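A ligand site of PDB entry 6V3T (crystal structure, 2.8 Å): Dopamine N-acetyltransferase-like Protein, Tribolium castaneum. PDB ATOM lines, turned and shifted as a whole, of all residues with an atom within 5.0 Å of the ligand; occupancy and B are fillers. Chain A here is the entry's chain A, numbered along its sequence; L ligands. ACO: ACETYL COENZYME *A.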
ATOM      1  N   PHE A  22      -9.412  20.438  19.194  1.00  0.00           N
ATOM      2  CA  PHE A  22      -7.946  20.202  19.227  1.00  0.00           C
ATOM      3  C   PHE A  22      -7.164  21.481  18.951  1.00  0.00           C
ATOM      4  O   PHE A  22      -6.034  21.501  19.398  1.00  0.00           O
ATOM      5  CB  PHE A  22      -7.519  19.057  18.304  1.00  0.00           C
ATOM      6  CG  PHE A  22      -6.084  18.654  18.541  1.00  0.00           C
ATOM      7  CD1 PHE A  22      -5.674  18.233  19.779  1.00  0.00           C
ATOM      8  CD2 PHE A  22      -5.130  18.763  17.544  1.00  0.00           C
ATOM      9  CE1 PHE A  22      -4.359  17.852  20.006  1.00  0.00           C
ATOM     10  CE2 PHE A  22      -3.810  18.401  17.783  1.00  0.00           C
ATOM     11  CZ  PHE A  22      -3.424  17.965  19.020  1.00  0.00           C
ATOM     12  N   ASP A  24      -6.896  24.410  20.453  1.00  0.00           N
ATOM     13  CA  ASP A  24      -6.361  25.048  21.691  1.00  0.00           C
ATOM     14  C   ASP A  24      -5.231  24.189  22.275  1.00  0.00           C
ATOM     15  O   ASP A  24      -4.898  24.373  23.456  1.00  0.00           O
ATOM     16  CB  ASP A  24      -7.458  25.365  22.726  1.00  0.00           C
ATOM     17  CG  ASP A  24      -8.607  24.374  22.788  1.00  0.00           C
ATOM     18  OD1 ASP A  24      -8.422  23.243  22.278  1.00  0.00           O
ATOM     19  OD2 ASP A  24      -9.671  24.728  23.348  1.00  0.00           O
ATOM     20  N   GLU A  25      -4.615  23.338  21.459  1.00  0.00           N
ATOM     21  CA  GLU A  25      -3.391  22.610  21.832  1.00  0.00           C
ATOM     22  C   GLU A  25      -2.297  23.654  22.050  1.00  0.00           C
ATOM     23  O   GLU A  25      -2.180  24.579  21.278  1.00  0.00           O
ATOM     24  CB  GLU A  25      -3.075  21.584  20.750  1.00  0.00           C
ATOM     25  CG  GLU A  25      -1.965  20.630  21.111  1.00  0.00           C
ATOM     26  CD  GLU A  25      -0.589  21.089  20.685  1.00  0.00           C
ATOM     27  OE1 GLU A  25      -0.515  21.975  19.815  1.00  0.00           O
ATOM     28  OE2 GLU A  25       0.395  20.575  21.236  1.00  0.00           O
ATOM     29  N   PRO A  26      -1.506  23.546  23.130  1.00  0.00           N
ATOM     30  CA  PRO A  26      -0.464  24.527  23.449  1.00  0.00           C
ATOM     31  C   PRO A  26       0.437  24.992  22.296  1.00  0.00           C
ATOM     32  O   PRO A  26       0.478  26.164  22.047  1.00  0.00           O
ATOM     33  CB  PRO A  26       0.404  23.784  24.474  1.00  0.00           C
ATOM     34  CG  PRO A  26      -0.578  22.893  25.180  1.00  0.00           C
ATOM     35  CD  PRO A  26      -1.575  22.472  24.132  1.00  0.00           C
ATOM     36  N   LEU A  27       1.172  24.081  21.665  1.00  0.00           N
ATOM     37  CA  LEU A  27       2.114  24.419  20.570  1.00  0.00           C
ATOM     38  C   LEU A  27       1.367  25.165  19.464  1.00  0.00           C
ATOM     39  O   LEU A  27       1.743  26.296  19.173  1.00  0.00           O
ATOM     40  CB  LEU A  27       2.735  23.144  20.028  1.00  0.00           C
ATOM     41  CG  LEU A  27       3.795  23.366  18.955  1.00  0.00           C
ATOM     42  CD1 LEU A  27       4.790  24.414  19.408  1.00  0.00           C
ATOM     43  CD2 LEU A  27       4.487  22.055  18.616  1.00  0.00           C
ATOM     44  N   ASN A  28       0.346  24.524  18.898  1.00  0.00           N
ATOM     45  CA  ASN A  28      -0.570  25.070  17.864  1.00  0.00           C
ATOM     46  C   ASN A  28      -0.885  26.519  18.202  1.00  0.00           C
ATOM     47  O   ASN A  28      -0.679  27.377  17.338  1.00  0.00           O
ATOM     48  CB  ASN A  28      -1.857  24.258  17.789  1.00  0.00           C
ATOM     49  CG  ASN A  28      -2.887  24.873  16.865  1.00  0.00           C
ATOM     50  OD1 ASN A  28      -3.241  26.024  17.012  1.00  0.00           O
ATOM     51  ND2 ASN A  28      -3.375  24.101  15.920  1.00  0.00           N
ATOM     52  N   LEU A  43      -3.172  19.048   8.525  1.00  0.00           N
ATOM     53  CA  LEU A  43      -2.987  18.017   9.575  1.00  0.00           C
ATOM     54  C   LEU A  43      -3.986  16.893   9.340  1.00  0.00           C
ATOM     55  O   LEU A  43      -3.578  15.737   9.461  1.00  0.00           O
ATOM     56  CB  LEU A  43      -3.231  18.628  10.957  1.00  0.00           C
ATOM     57  CG  LEU A  43      -2.052  19.405  11.506  1.00  0.00           C
ATOM     58  CD1 LEU A  43      -1.973  20.761  10.833  1.00  0.00           C
ATOM     59  CD2 LEU A  43      -2.147  19.542  13.013  1.00  0.00           C
ATOM     60  N   ILE A  99       5.999  24.405  13.895  1.00  0.00           N
ATOM     61  CA  ILE A  99       5.450  23.281  14.695  1.00  0.00           C
ATOM     62  C   ILE A  99       6.269  22.019  14.396  1.00  0.00           C
ATOM     63  O   ILE A  99       6.973  21.540  15.300  1.00  0.00           O
ATOM     64  CB  ILE A  99       3.965  23.042  14.390  1.00  0.00           C
ATOM     65  CG1 ILE A  99       3.093  24.227  14.829  1.00  0.00           C
ATOM     66  CG2 ILE A  99       3.509  21.743  15.039  1.00  0.00           C
ATOM     67  CD1 ILE A  99       1.603  23.985  14.706  1.00  0.00           C
ATOM     68  N   PHE A 100       6.177  21.493  13.185  1.00  0.00           N
ATOM     69  CA  PHE A 100       6.615  20.112  12.875  1.00  0.00           C
ATOM     70  C   PHE A 100       8.130  20.042  12.707  1.00  0.00           C
ATOM     71  O   PHE A 100       8.716  18.946  12.880  1.00  0.00           O
ATOM     72  CB  PHE A 100       5.858  19.602  11.675  1.00  0.00           C
ATOM     73  CG  PHE A 100       4.425  19.282  11.987  1.00  0.00           C
ATOM     74  CD1 PHE A 100       4.114  18.239  12.833  1.00  0.00           C
ATOM     75  CD2 PHE A 100       3.388  20.011  11.468  1.00  0.00           C
ATOM     76  CE1 PHE A 100       2.800  17.926  13.135  1.00  0.00           C
ATOM     77  CE2 PHE A 100       2.074  19.695  11.756  1.00  0.00           C
ATOM     78  CZ  PHE A 100       1.783  18.649  12.591  1.00  0.00           C
ATOM     79  N   LEU A 103       9.109  19.333  16.290  1.00  0.00           N
ATOM     80  CA  LEU A 103       8.738  17.927  16.614  1.00  0.00           C
ATOM     81  C   LEU A 103       9.735  16.973  15.955  1.00  0.00           C
ATOM     82  O   LEU A 103      10.369  16.165  16.670  1.00  0.00           O
ATOM     83  CB  LEU A 103       7.306  17.680  16.158  1.00  0.00           C
ATOM     84  CG  LEU A 103       6.238  18.449  16.947  1.00  0.00           C
ATOM     85  CD1 LEU A 103       4.846  18.021  16.531  1.00  0.00           C
ATOM     86  CD2 LEU A 103       6.404  18.237  18.443  1.00  0.00           C
ATOM     87  N   ARG A 125      -0.047   9.981  19.323  1.00  0.00           N
ATOM     88  CA  ARG A 125       0.309  11.170  18.526  1.00  0.00           C
ATOM     89  C   ARG A 125      -0.635  12.309  18.864  1.00  0.00           C
ATOM     90  O   ARG A 125      -0.135  13.456  18.989  1.00  0.00           O
ATOM     91  CB  ARG A 125       0.216  10.864  17.024  1.00  0.00           C
ATOM     92  CG  ARG A 125       1.168   9.768  16.606  1.00  0.00           C
ATOM     93  CD  ARG A 125       1.164   9.563  15.109  1.00  0.00           C
ATOM     94  NE  ARG A 125       2.327   8.818  14.695  1.00  0.00           N
ATOM     95  CZ  ARG A 125       2.448   8.153  13.564  1.00  0.00           C
ATOM     96  NH1 ARG A 125       1.445   8.120  12.692  1.00  0.00           N
ATOM     97  NH2 ARG A 125       3.583   7.527  13.305  1.00  0.00           N
ATOM     98  N   ILE A 126      -1.922  12.030  18.959  1.00  0.00           N
ATOM     99  CA  ILE A 126      -2.963  13.083  19.188  1.00  0.00           C
ATOM    100  C   ILE A 126      -3.916  12.635  20.295  1.00  0.00           C
ATOM    101  O   ILE A 126      -4.522  11.571  20.178  1.00  0.00           O
ATOM    102  CB  ILE A 126      -3.686  13.420  17.874  1.00  0.00           C
ATOM    103  CG1 ILE A 126      -2.754  14.185  16.934  1.00  0.00           C
ATOM    104  CG2 ILE A 126      -4.973  14.193  18.175  1.00  0.00           C
ATOM    105  CD1 ILE A 126      -3.456  15.036  15.905  1.00  0.00           C
ATOM    106  N   LEU A 127      -4.040  13.473  21.319  1.00  0.00           N
ATOM    107  CA  LEU A 127      -4.900  13.220  22.508  1.00  0.00           C
ATOM    108  C   LEU A 127      -5.911  14.359  22.635  1.00  0.00           C
ATOM    109  O   LEU A 127      -5.494  15.469  23.027  1.00  0.00           O
ATOM    110  CB  LEU A 127      -3.979  13.128  23.721  1.00  0.00           C
ATOM    111  CG  LEU A 127      -4.583  12.494  24.969  1.00  0.00           C
ATOM    112  CD1 LEU A 127      -5.442  11.299  24.604  1.00  0.00           C
ATOM    113  CD2 LEU A 127      -3.491  12.096  25.951  1.00  0.00           C
ATOM    114  N   SER A 128      -7.178  14.097  22.294  1.00  0.00           N
ATOM    115  CA  SER A 128      -8.284  15.091  22.353  1.00  0.00           C
ATOM    116  C   SER A 128      -9.393  14.629  23.302  1.00  0.00           C
ATOM    117  O   SER A 128      -9.900  13.493  23.145  1.00  0.00           O
ATOM    118  CB  SER A 128      -8.859  15.372  20.995  1.00  0.00           C
ATOM    119  OG  SER A 128      -9.896  16.345  21.088  1.00  0.00           O
ATOM    120  N   VAL A 129      -9.755  15.509  24.248  1.00  0.00           N
ATOM    121  CA  VAL A 129     -10.961  15.394  25.110  1.00  0.00           C
ATOM    122  C   VAL A 129     -11.777  16.658  24.865  1.00  0.00           C
ATOM    123  O   VAL A 129     -11.186  17.721  25.009  1.00  0.00           O
ATOM    124  CB  VAL A 129     -10.557  15.294  26.588  1.00  0.00           C
ATOM    125  CG1 VAL A 129     -11.765  15.169  27.502  1.00  0.00           C
ATOM    126  CG2 VAL A 129      -9.594  14.156  26.802  1.00  0.00           C
ATOM    127  N   ARG A 134     -14.013  17.725  29.454  1.00  0.00           N
ATOM    128  CA  ARG A 134     -12.595  17.869  29.864  1.00  0.00           C
ATOM    129  C   ARG A 134     -12.494  17.991  31.373  1.00  0.00           C
ATOM    130  O   ARG A 134     -13.255  18.765  31.949  1.00  0.00           O
ATOM    131  CB  ARG A 134     -12.007  19.110  29.198  1.00  0.00           C
ATOM    132  CG  ARG A 134     -10.493  19.240  29.295  1.00  0.00           C
ATOM    133  CD  ARG A 134      -9.984  20.263  28.293  1.00  0.00           C
ATOM    134  NE  ARG A 134     -10.336  19.899  26.920  1.00  0.00           N
ATOM    135  CZ  ARG A 134     -10.170  20.682  25.862  1.00  0.00           C
ATOM    136  NH1 ARG A 134      -9.661  21.898  26.004  1.00  0.00           N
ATOM    137  NH2 ARG A 134     -10.517  20.255  24.647  1.00  0.00           N
ATOM    138  N   GLY A 135     -11.543  17.284  31.987  1.00  0.00           N
ATOM    139  CA  GLY A 135     -11.237  17.378  33.430  1.00  0.00           C
ATOM    140  C   GLY A 135     -11.887  16.272  34.252  1.00  0.00           C
ATOM    141  O   GLY A 135     -11.923  16.403  35.469  1.00  0.00           O
ATOM    142  N   ARG A 136     -12.349  15.194  33.624  1.00  0.00           N
ATOM    143  CA  ARG A 136     -12.988  14.069  34.349  1.00  0.00           C
ATOM    144  C   ARG A 136     -12.112  12.824  34.213  1.00  0.00           C
ATOM    145  O   ARG A 136     -12.664  11.709  34.235  1.00  0.00           O
ATOM    146  CB  ARG A 136     -14.411  13.835  33.833  1.00  0.00           C
ATOM    147  CG  ARG A 136     -15.195  15.099  33.519  1.00  0.00           C
ATOM    148  CD  ARG A 136     -16.660  14.840  33.185  1.00  0.00           C
ATOM    149  NE  ARG A 136     -17.048  13.432  33.218  1.00  0.00           N
ATOM    150  CZ  ARG A 136     -18.214  12.943  32.831  1.00  0.00           C
ATOM    151  NH1 ARG A 136     -18.460  11.642  32.909  1.00  0.00           N
ATOM    152  NH2 ARG A 136     -19.171  13.746  32.371  1.00  0.00           N
ATOM    153  N   GLY A 137     -10.789  12.998  34.092  1.00  0.00           N
ATOM    154  CA  GLY A 137      -9.798  11.908  34.017  1.00  0.00           C
ATOM    155  C   GLY A 137     -10.002  11.026  32.785  1.00  0.00           C
ATOM    156  O   GLY A 137      -9.690   9.823  32.853  1.00  0.00           O
ATOM    157  N   ILE A 138     -10.501  11.587  31.691  1.00  0.00           N
ATOM    158  CA  ILE A 138     -10.790  10.807  30.450  1.00  0.00           C
ATOM    159  C   ILE A 138      -9.479  10.549  29.703  1.00  0.00           C
ATOM    160  O   ILE A 138      -9.255   9.406  29.286  1.00  0.00           O
ATOM    161  CB  ILE A 138     -11.817  11.545  29.583  1.00  0.00           C
ATOM    162  CG1 ILE A 138     -13.080  11.848  30.392  1.00  0.00           C
ATOM    163  CG2 ILE A 138     -12.096  10.762  28.308  1.00  0.00           C
ATOM    164  CD1 ILE A 138     -14.333  12.021  29.597  1.00  0.00           C
ATOM    165  N   ALA A 139      -8.653  11.572  29.533  1.00  0.00           N
ATOM    166  CA  ALA A 139      -7.331  11.462  28.873  1.00  0.00           C
ATOM    167  C   ALA A 139      -6.558  10.331  29.537  1.00  0.00           C
ATOM    168  O   ALA A 139      -6.143   9.393  28.840  1.00  0.00           O
ATOM    169  CB  ALA A 139      -6.590  12.758  28.981  1.00  0.00           C
ATOM    170  N   LYS A 140      -6.394  10.428  30.855  1.00  0.00           N
ATOM    171  CA  LYS A 140      -5.682   9.419  31.670  1.00  0.00           C
ATOM    172  C   LYS A 140      -6.163   8.011  31.279  1.00  0.00           C
ATOM    173  O   LYS A 140      -5.326   7.100  31.282  1.00  0.00           O
ATOM    174  CB  LYS A 140      -5.890   9.676  33.162  1.00  0.00           C
ATOM    175  CG  LYS A 140      -4.872  10.617  33.791  1.00  0.00           C
ATOM    176  CD  LYS A 140      -5.223  11.049  35.182  1.00  0.00           C
ATOM    177  CE  LYS A 140      -4.509  10.234  36.233  1.00  0.00           C
ATOM    178  NZ  LYS A 140      -5.171  10.370  37.555  1.00  0.00           N
ATOM    179  N   VAL A 160       5.327   9.466  23.233  1.00  0.00           N
ATOM    180  CA  VAL A 160       4.314  10.551  23.154  1.00  0.00           C
ATOM    181  C   VAL A 160       5.024  11.911  23.079  1.00  0.00           C
ATOM    182  O   VAL A 160       5.925  12.187  23.928  1.00  0.00           O
ATOM    183  CB  VAL A 160       3.334  10.515  24.352  1.00  0.00           C
ATOM    184  CG1 VAL A 160       4.066  10.581  25.687  1.00  0.00           C
ATOM    185  CG2 VAL A 160       2.285  11.605  24.239  1.00  0.00           C
ATOM    186  N   ASP A 161       4.622  12.728  22.105  1.00  0.00           N
ATOM    187  CA  ASP A 161       5.108  14.121  21.977  1.00  0.00           C
ATOM    188  C   ASP A 161       4.257  14.953  22.930  1.00  0.00           C
ATOM    189  O   ASP A 161       3.209  15.436  22.495  1.00  0.00           O
ATOM    190  CB  ASP A 161       5.066  14.610  20.535  1.00  0.00           C
ATOM    191  CG  ASP A 161       6.265  14.165  19.732  1.00  0.00           C
ATOM    192  OD1 ASP A 161       7.385  14.620  20.048  1.00  0.00           O
ATOM    193  OD2 ASP A 161       6.075  13.360  18.812  1.00  0.00           O
ATOM    194  N   THR A 163       3.281  17.826  24.510  1.00  0.00           N
ATOM    195  CA  THR A 163       3.365  19.302  24.372  1.00  0.00           C
ATOM    196  C   THR A 163       2.568  19.961  25.496  1.00  0.00           C
ATOM    197  O   THR A 163       2.979  21.027  25.968  1.00  0.00           O
ATOM    198  CB  THR A 163       2.800  19.735  23.029  1.00  0.00           C
ATOM    199  OG1 THR A 163       1.436  19.336  23.110  1.00  0.00           O
ATOM    200  CG2 THR A 163       3.487  19.082  21.856  1.00  0.00           C
ATOM    201  N   SER A 164       1.435  19.353  25.854  1.00  0.00           N
ATOM    202  CA  SER A 164       0.589  19.774  26.998  1.00  0.00           C
ATOM    203  C   SER A 164       1.185  19.175  28.276  1.00  0.00           C
ATOM    204  O   SER A 164       1.565  18.009  28.237  1.00  0.00           O
ATOM    205  CB  SER A 164      -0.827  19.321  26.809  1.00  0.00           C
ATOM    206  OG  SER A 164      -1.668  19.830  27.826  1.00  0.00           O
ATOM    207  N   PHE A 166      -0.514  18.761  31.006  1.00  0.00           N
ATOM    208  CA  PHE A 166      -1.566  17.804  31.435  1.00  0.00           C
ATOM    209  C   PHE A 166      -1.224  16.431  30.874  1.00  0.00           C
ATOM    210  O   PHE A 166      -1.303  15.456  31.595  1.00  0.00           O
ATOM    211  CB  PHE A 166      -2.946  18.239  30.973  1.00  0.00           C
ATOM    212  CG  PHE A 166      -3.258  19.684  31.284  1.00  0.00           C
ATOM    213  CD1 PHE A 166      -2.575  20.347  32.286  1.00  0.00           C
ATOM    214  CD2 PHE A 166      -4.222  20.371  30.578  1.00  0.00           C
ATOM    215  CE1 PHE A 166      -2.849  21.685  32.557  1.00  0.00           C
ATOM    216  CE2 PHE A 166      -4.508  21.701  30.849  1.00  0.00           C
ATOM    217  CZ  PHE A 166      -3.819  22.354  31.840  1.00  0.00           C
ATOM    218  N   THR A 167      -0.812  16.402  29.613  1.00  0.00           N
ATOM    219  CA  THR A 167      -0.386  15.163  28.919  1.00  0.00           C
ATOM    220  C   THR A 167       0.889  14.630  29.563  1.00  0.00           C
ATOM    221  O   THR A 167       1.086  13.412  29.513  1.00  0.00           O
ATOM    222  CB  THR A 167      -0.131  15.397  27.429  1.00  0.00           C
ATOM    223  OG1 THR A 167      -1.403  15.619  26.817  1.00  0.00           O
ATOM    224  CG2 THR A 167       0.568  14.240  26.755  1.00  0.00           C
ATOM    225  N   ARG A 169       1.581  14.993  32.756  1.00  0.00           N
ATOM    226  CA  ARG A 169       1.079  14.451  34.034  1.00  0.00           C
ATOM    227  C   ARG A 169       0.547  13.049  33.825  1.00  0.00           C
ATOM    228  O   ARG A 169       0.901  12.186  34.592  1.00  0.00           O
ATOM    229  CB  ARG A 169      -0.035  15.323  34.595  1.00  0.00           C
ATOM    230  CG  ARG A 169       0.457  16.341  35.607  1.00  0.00           C
ATOM    231  CD  ARG A 169      -0.481  17.521  35.590  1.00  0.00           C
ATOM    232  NE  ARG A 169      -0.237  18.638  36.491  1.00  0.00           N
ATOM    233  CZ  ARG A 169       0.943  19.078  36.932  1.00  0.00           C
ATOM    234  NH1 ARG A 169       2.084  18.498  36.606  1.00  0.00           N
ATOM    235  NH2 ARG A 169       0.956  20.126  37.726  1.00  0.00           N
ATOM    236  N   ALA A 170      -0.320  12.867  32.852  1.00  0.00           N
ATOM    237  CA  ALA A 170      -0.909  11.548  32.541  1.00  0.00           C
ATOM    238  C   ALA A 170       0.248  10.564  32.362  1.00  0.00           C
ATOM    239  O   ALA A 170       0.278   9.540  33.017  1.00  0.00           O
ATOM    240  CB  ALA A 170      -1.757  11.653  31.303  1.00  0.00           C
ATOM    241  N   CYS A 173       1.954   9.629  35.409  1.00  0.00           N
ATOM    242  CA  CYS A 173       1.096   8.766  36.261  1.00  0.00           C
ATOM    243  C   CYS A 173       1.167   7.311  35.810  1.00  0.00           C
ATOM    244  O   CYS A 173       1.021   6.465  36.679  1.00  0.00           O
ATOM    245  CB  CYS A 173      -0.353   9.225  36.316  1.00  0.00           C
ATOM    246  SG  CYS A 173      -0.736  10.147  37.832  1.00  0.00           S
HETATM  247  N1A ACO L   1      -5.150  22.339  35.176  1.00  0.00           N
HETATM  248  C2A ACO L   1      -4.248  21.616  35.839  1.00  0.00           C
HETATM  249  N3A ACO L   1      -4.122  20.281  35.682  1.00  0.00           N
HETATM  250  C4A ACO L   1      -4.923  19.612  34.834  1.00  0.00           C
HETATM  251  C5A ACO L   1      -5.926  20.350  34.092  1.00  0.00           C
HETATM  252  C6A ACO L   1      -6.005  21.789  34.314  1.00  0.00           C
HETATM  253  N6A ACO L   1      -6.922  22.507  33.666  1.00  0.00           N
HETATM  254  N7A ACO L   1      -6.575  19.463  33.341  1.00  0.00           N
HETATM  255  C8A ACO L   1      -6.034  18.249  33.575  1.00  0.00           C
HETATM  256  N9A ACO L   1      -5.065  18.354  34.480  1.00  0.00           N
HETATM  257  C1B ACO L   1      -4.247  17.228  34.930  1.00  0.00           C
HETATM  258  C2B ACO L   1      -4.903  16.414  36.012  1.00  0.00           C
HETATM  259  O2B ACO L   1      -4.505  16.853  37.296  1.00  0.00           O
HETATM  260  C3B ACO L   1      -4.333  15.047  35.693  1.00  0.00           C
HETATM  261  O3B ACO L   1      -3.036  14.950  36.224  1.00  0.00           O
HETATM  262  P3B ACO L   1      -2.819  14.105  37.553  1.00  0.00           P
HETATM  263  O7A ACO L   1      -1.647  14.770  38.231  1.00  0.00           O
HETATM  264  O8A ACO L   1      -4.158  14.355  38.241  1.00  0.00           O
HETATM  265  O9A ACO L   1      -2.552  12.719  36.972  1.00  0.00           O
HETATM  266  C4B ACO L   1      -4.180  15.008  34.202  1.00  0.00           C
HETATM  267  O4B ACO L   1      -4.154  16.358  33.807  1.00  0.00           O
HETATM  268  C5B ACO L   1      -5.307  14.308  33.513  1.00  0.00           C
HETATM  269  O5B ACO L   1      -6.435  15.141  33.370  1.00  0.00           O
HETATM  270  P1A ACO L   1      -7.566  14.572  32.416  1.00  0.00           P
HETATM  271  O1A ACO L   1      -7.507  13.059  32.453  1.00  0.00           O
HETATM  272  O2A ACO L   1      -8.890  15.238  32.618  1.00  0.00           O
HETATM  273  O3A ACO L   1      -7.030  15.139  31.021  1.00  0.00           O
HETATM  274  P2A ACO L   1      -8.050  15.934  30.078  1.00  0.00           P
HETATM  275  O4A ACO L   1      -9.282  15.054  29.936  1.00  0.00           O
HETATM  276  O5A ACO L   1      -8.252  17.318  30.638  1.00  0.00           O
HETATM  277  O6A ACO L   1      -7.065  16.098  28.769  1.00  0.00           O
HETATM  278  CBP ACO L   1      -6.133  17.721  27.065  1.00  0.00           C
HETATM  279  CCP ACO L   1      -7.345  16.971  27.645  1.00  0.00           C
HETATM  280  CDP ACO L   1      -4.887  16.884  27.294  1.00  0.00           C
HETATM  281  CEP ACO L   1      -6.085  19.046  27.794  1.00  0.00           C
HETATM  282  CAP ACO L   1      -6.279  18.052  25.526  1.00  0.00           C
HETATM  283  OAP ACO L   1      -7.244  19.096  25.366  1.00  0.00           O
HETATM  284  C9P ACO L   1      -4.998  18.488  24.725  1.00  0.00           C
HETATM  285  O9P ACO L   1      -4.748  19.681  24.545  1.00  0.00           O
HETATM  286  N8P ACO L   1      -4.187  17.517  24.194  1.00  0.00           N
HETATM  287  C7P ACO L   1      -2.931  17.772  23.484  1.00  0.00           C
HETATM  288  C6P ACO L   1      -1.717  16.949  23.975  1.00  0.00           C
HETATM  289  C5P ACO L   1      -0.879  16.320  22.872  1.00  0.00           C
HETATM  290  O5P ACO L   1      -0.753  15.124  22.789  1.00  0.00           O
HETATM  291  N4P ACO L   1      -0.254  17.146  22.038  1.00  0.00           N
HETATM  292  C3P ACO L   1       0.742  16.708  21.038  1.00  0.00           C
HETATM  293  C2P ACO L   1       0.449  17.026  19.551  1.00  0.00           C
HETATM  294  S1P ACO L   1       1.428  18.340  18.877  1.00  0.00           S
HETATM  295  C   ACO L   1       0.482  18.991  17.629  1.00  0.00           C
HETATM  296  O   ACO L   1      -0.215  18.257  16.937  1.00  0.00           O
HETATM  297  CH3 ACO L   1       0.481  20.459  17.332  1.00  0.00           C
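O of Leu 127 sits at hydrogen-bond distance from N8P of the ligand. N4P of the ligand lies within hydrogen-bond range of OG1 of Thr 163, at 3.0 Å. N of Gly 137 sits at hydrogen-bond distance from O2A of the ligand (3.3 Å). An oxygen (O1A) of the ligand sits at hydrogen-bond distance from the backbone NH (N) of Ala 139 (3.5 Å). O1A of the ligand is in hydrogen-bond range of N of Lys 140, 3.3 Å away. The side-chain amino group of Lys 140 lies within salt-bridge range of an oxygen (O9A) of the ligand (3.6 Å). The side-chain sulfur (SG) of Cys 173 lies within hydrogen-bond range of an oxygen (O9A) of the ligand (3.3 Å). N of Gly 135 lies close to O2A of the ligand, at 3.4 Å. The backbone NH (N) of Ile 138 lies within hydrogen-bond range of an oxygen (O1A) of the ligand (3.4 Å).
The side-chain hydroxyl (OG1) of Thr 163 sits at hydrogen-bond distance from the side-chain carboxylate (OE2) of Glu 25, 2.5 Å away. The backbone NH (N) of Asn 28 lies within hydrogen-bond range of the side-chain carboxylate (OE1) of Glu 25, at 2.8 Å. The side-chain carboxylate (OE1) of Glu 25 sits at hydrogen-bond distance from the backbone NH (N) of Leu 27, at 3.3 Å. The guanidinium group (NH2) of Arg 134 lies within hydrogen-bond range of the backbone carbonyl oxygen (O) of Val 129 (2.6 Å). OD2 of Asp 24 lies within salt-bridge range of NH1 of Arg 134 (3.9 Å).
The side-chain carboxylate (OE2) of Glu 25 sits close to a sulfur (S1P) of the ligand. Residues that only touch the ligand: Phe 22 (3.7 Å), Arg 125 (3.7 Å), Val 129 (3.3 Å), Arg 134 (3.2 Å), Arg 136 (3.6 Å), Asp 161 (3.1 Å), Ser 164 (3.8 Å), Phe 166 (3.3 Å), Thr 167 (3.2 Å) and Arg 169 (3.4 Å). Hydrophobic or aromatic side chains that line the ligand: Phe 22, Leu 127, Val 129, Ala 139 and Phe 166. Of the 31 residues printed, 19 come within 4 Å of the ligand.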
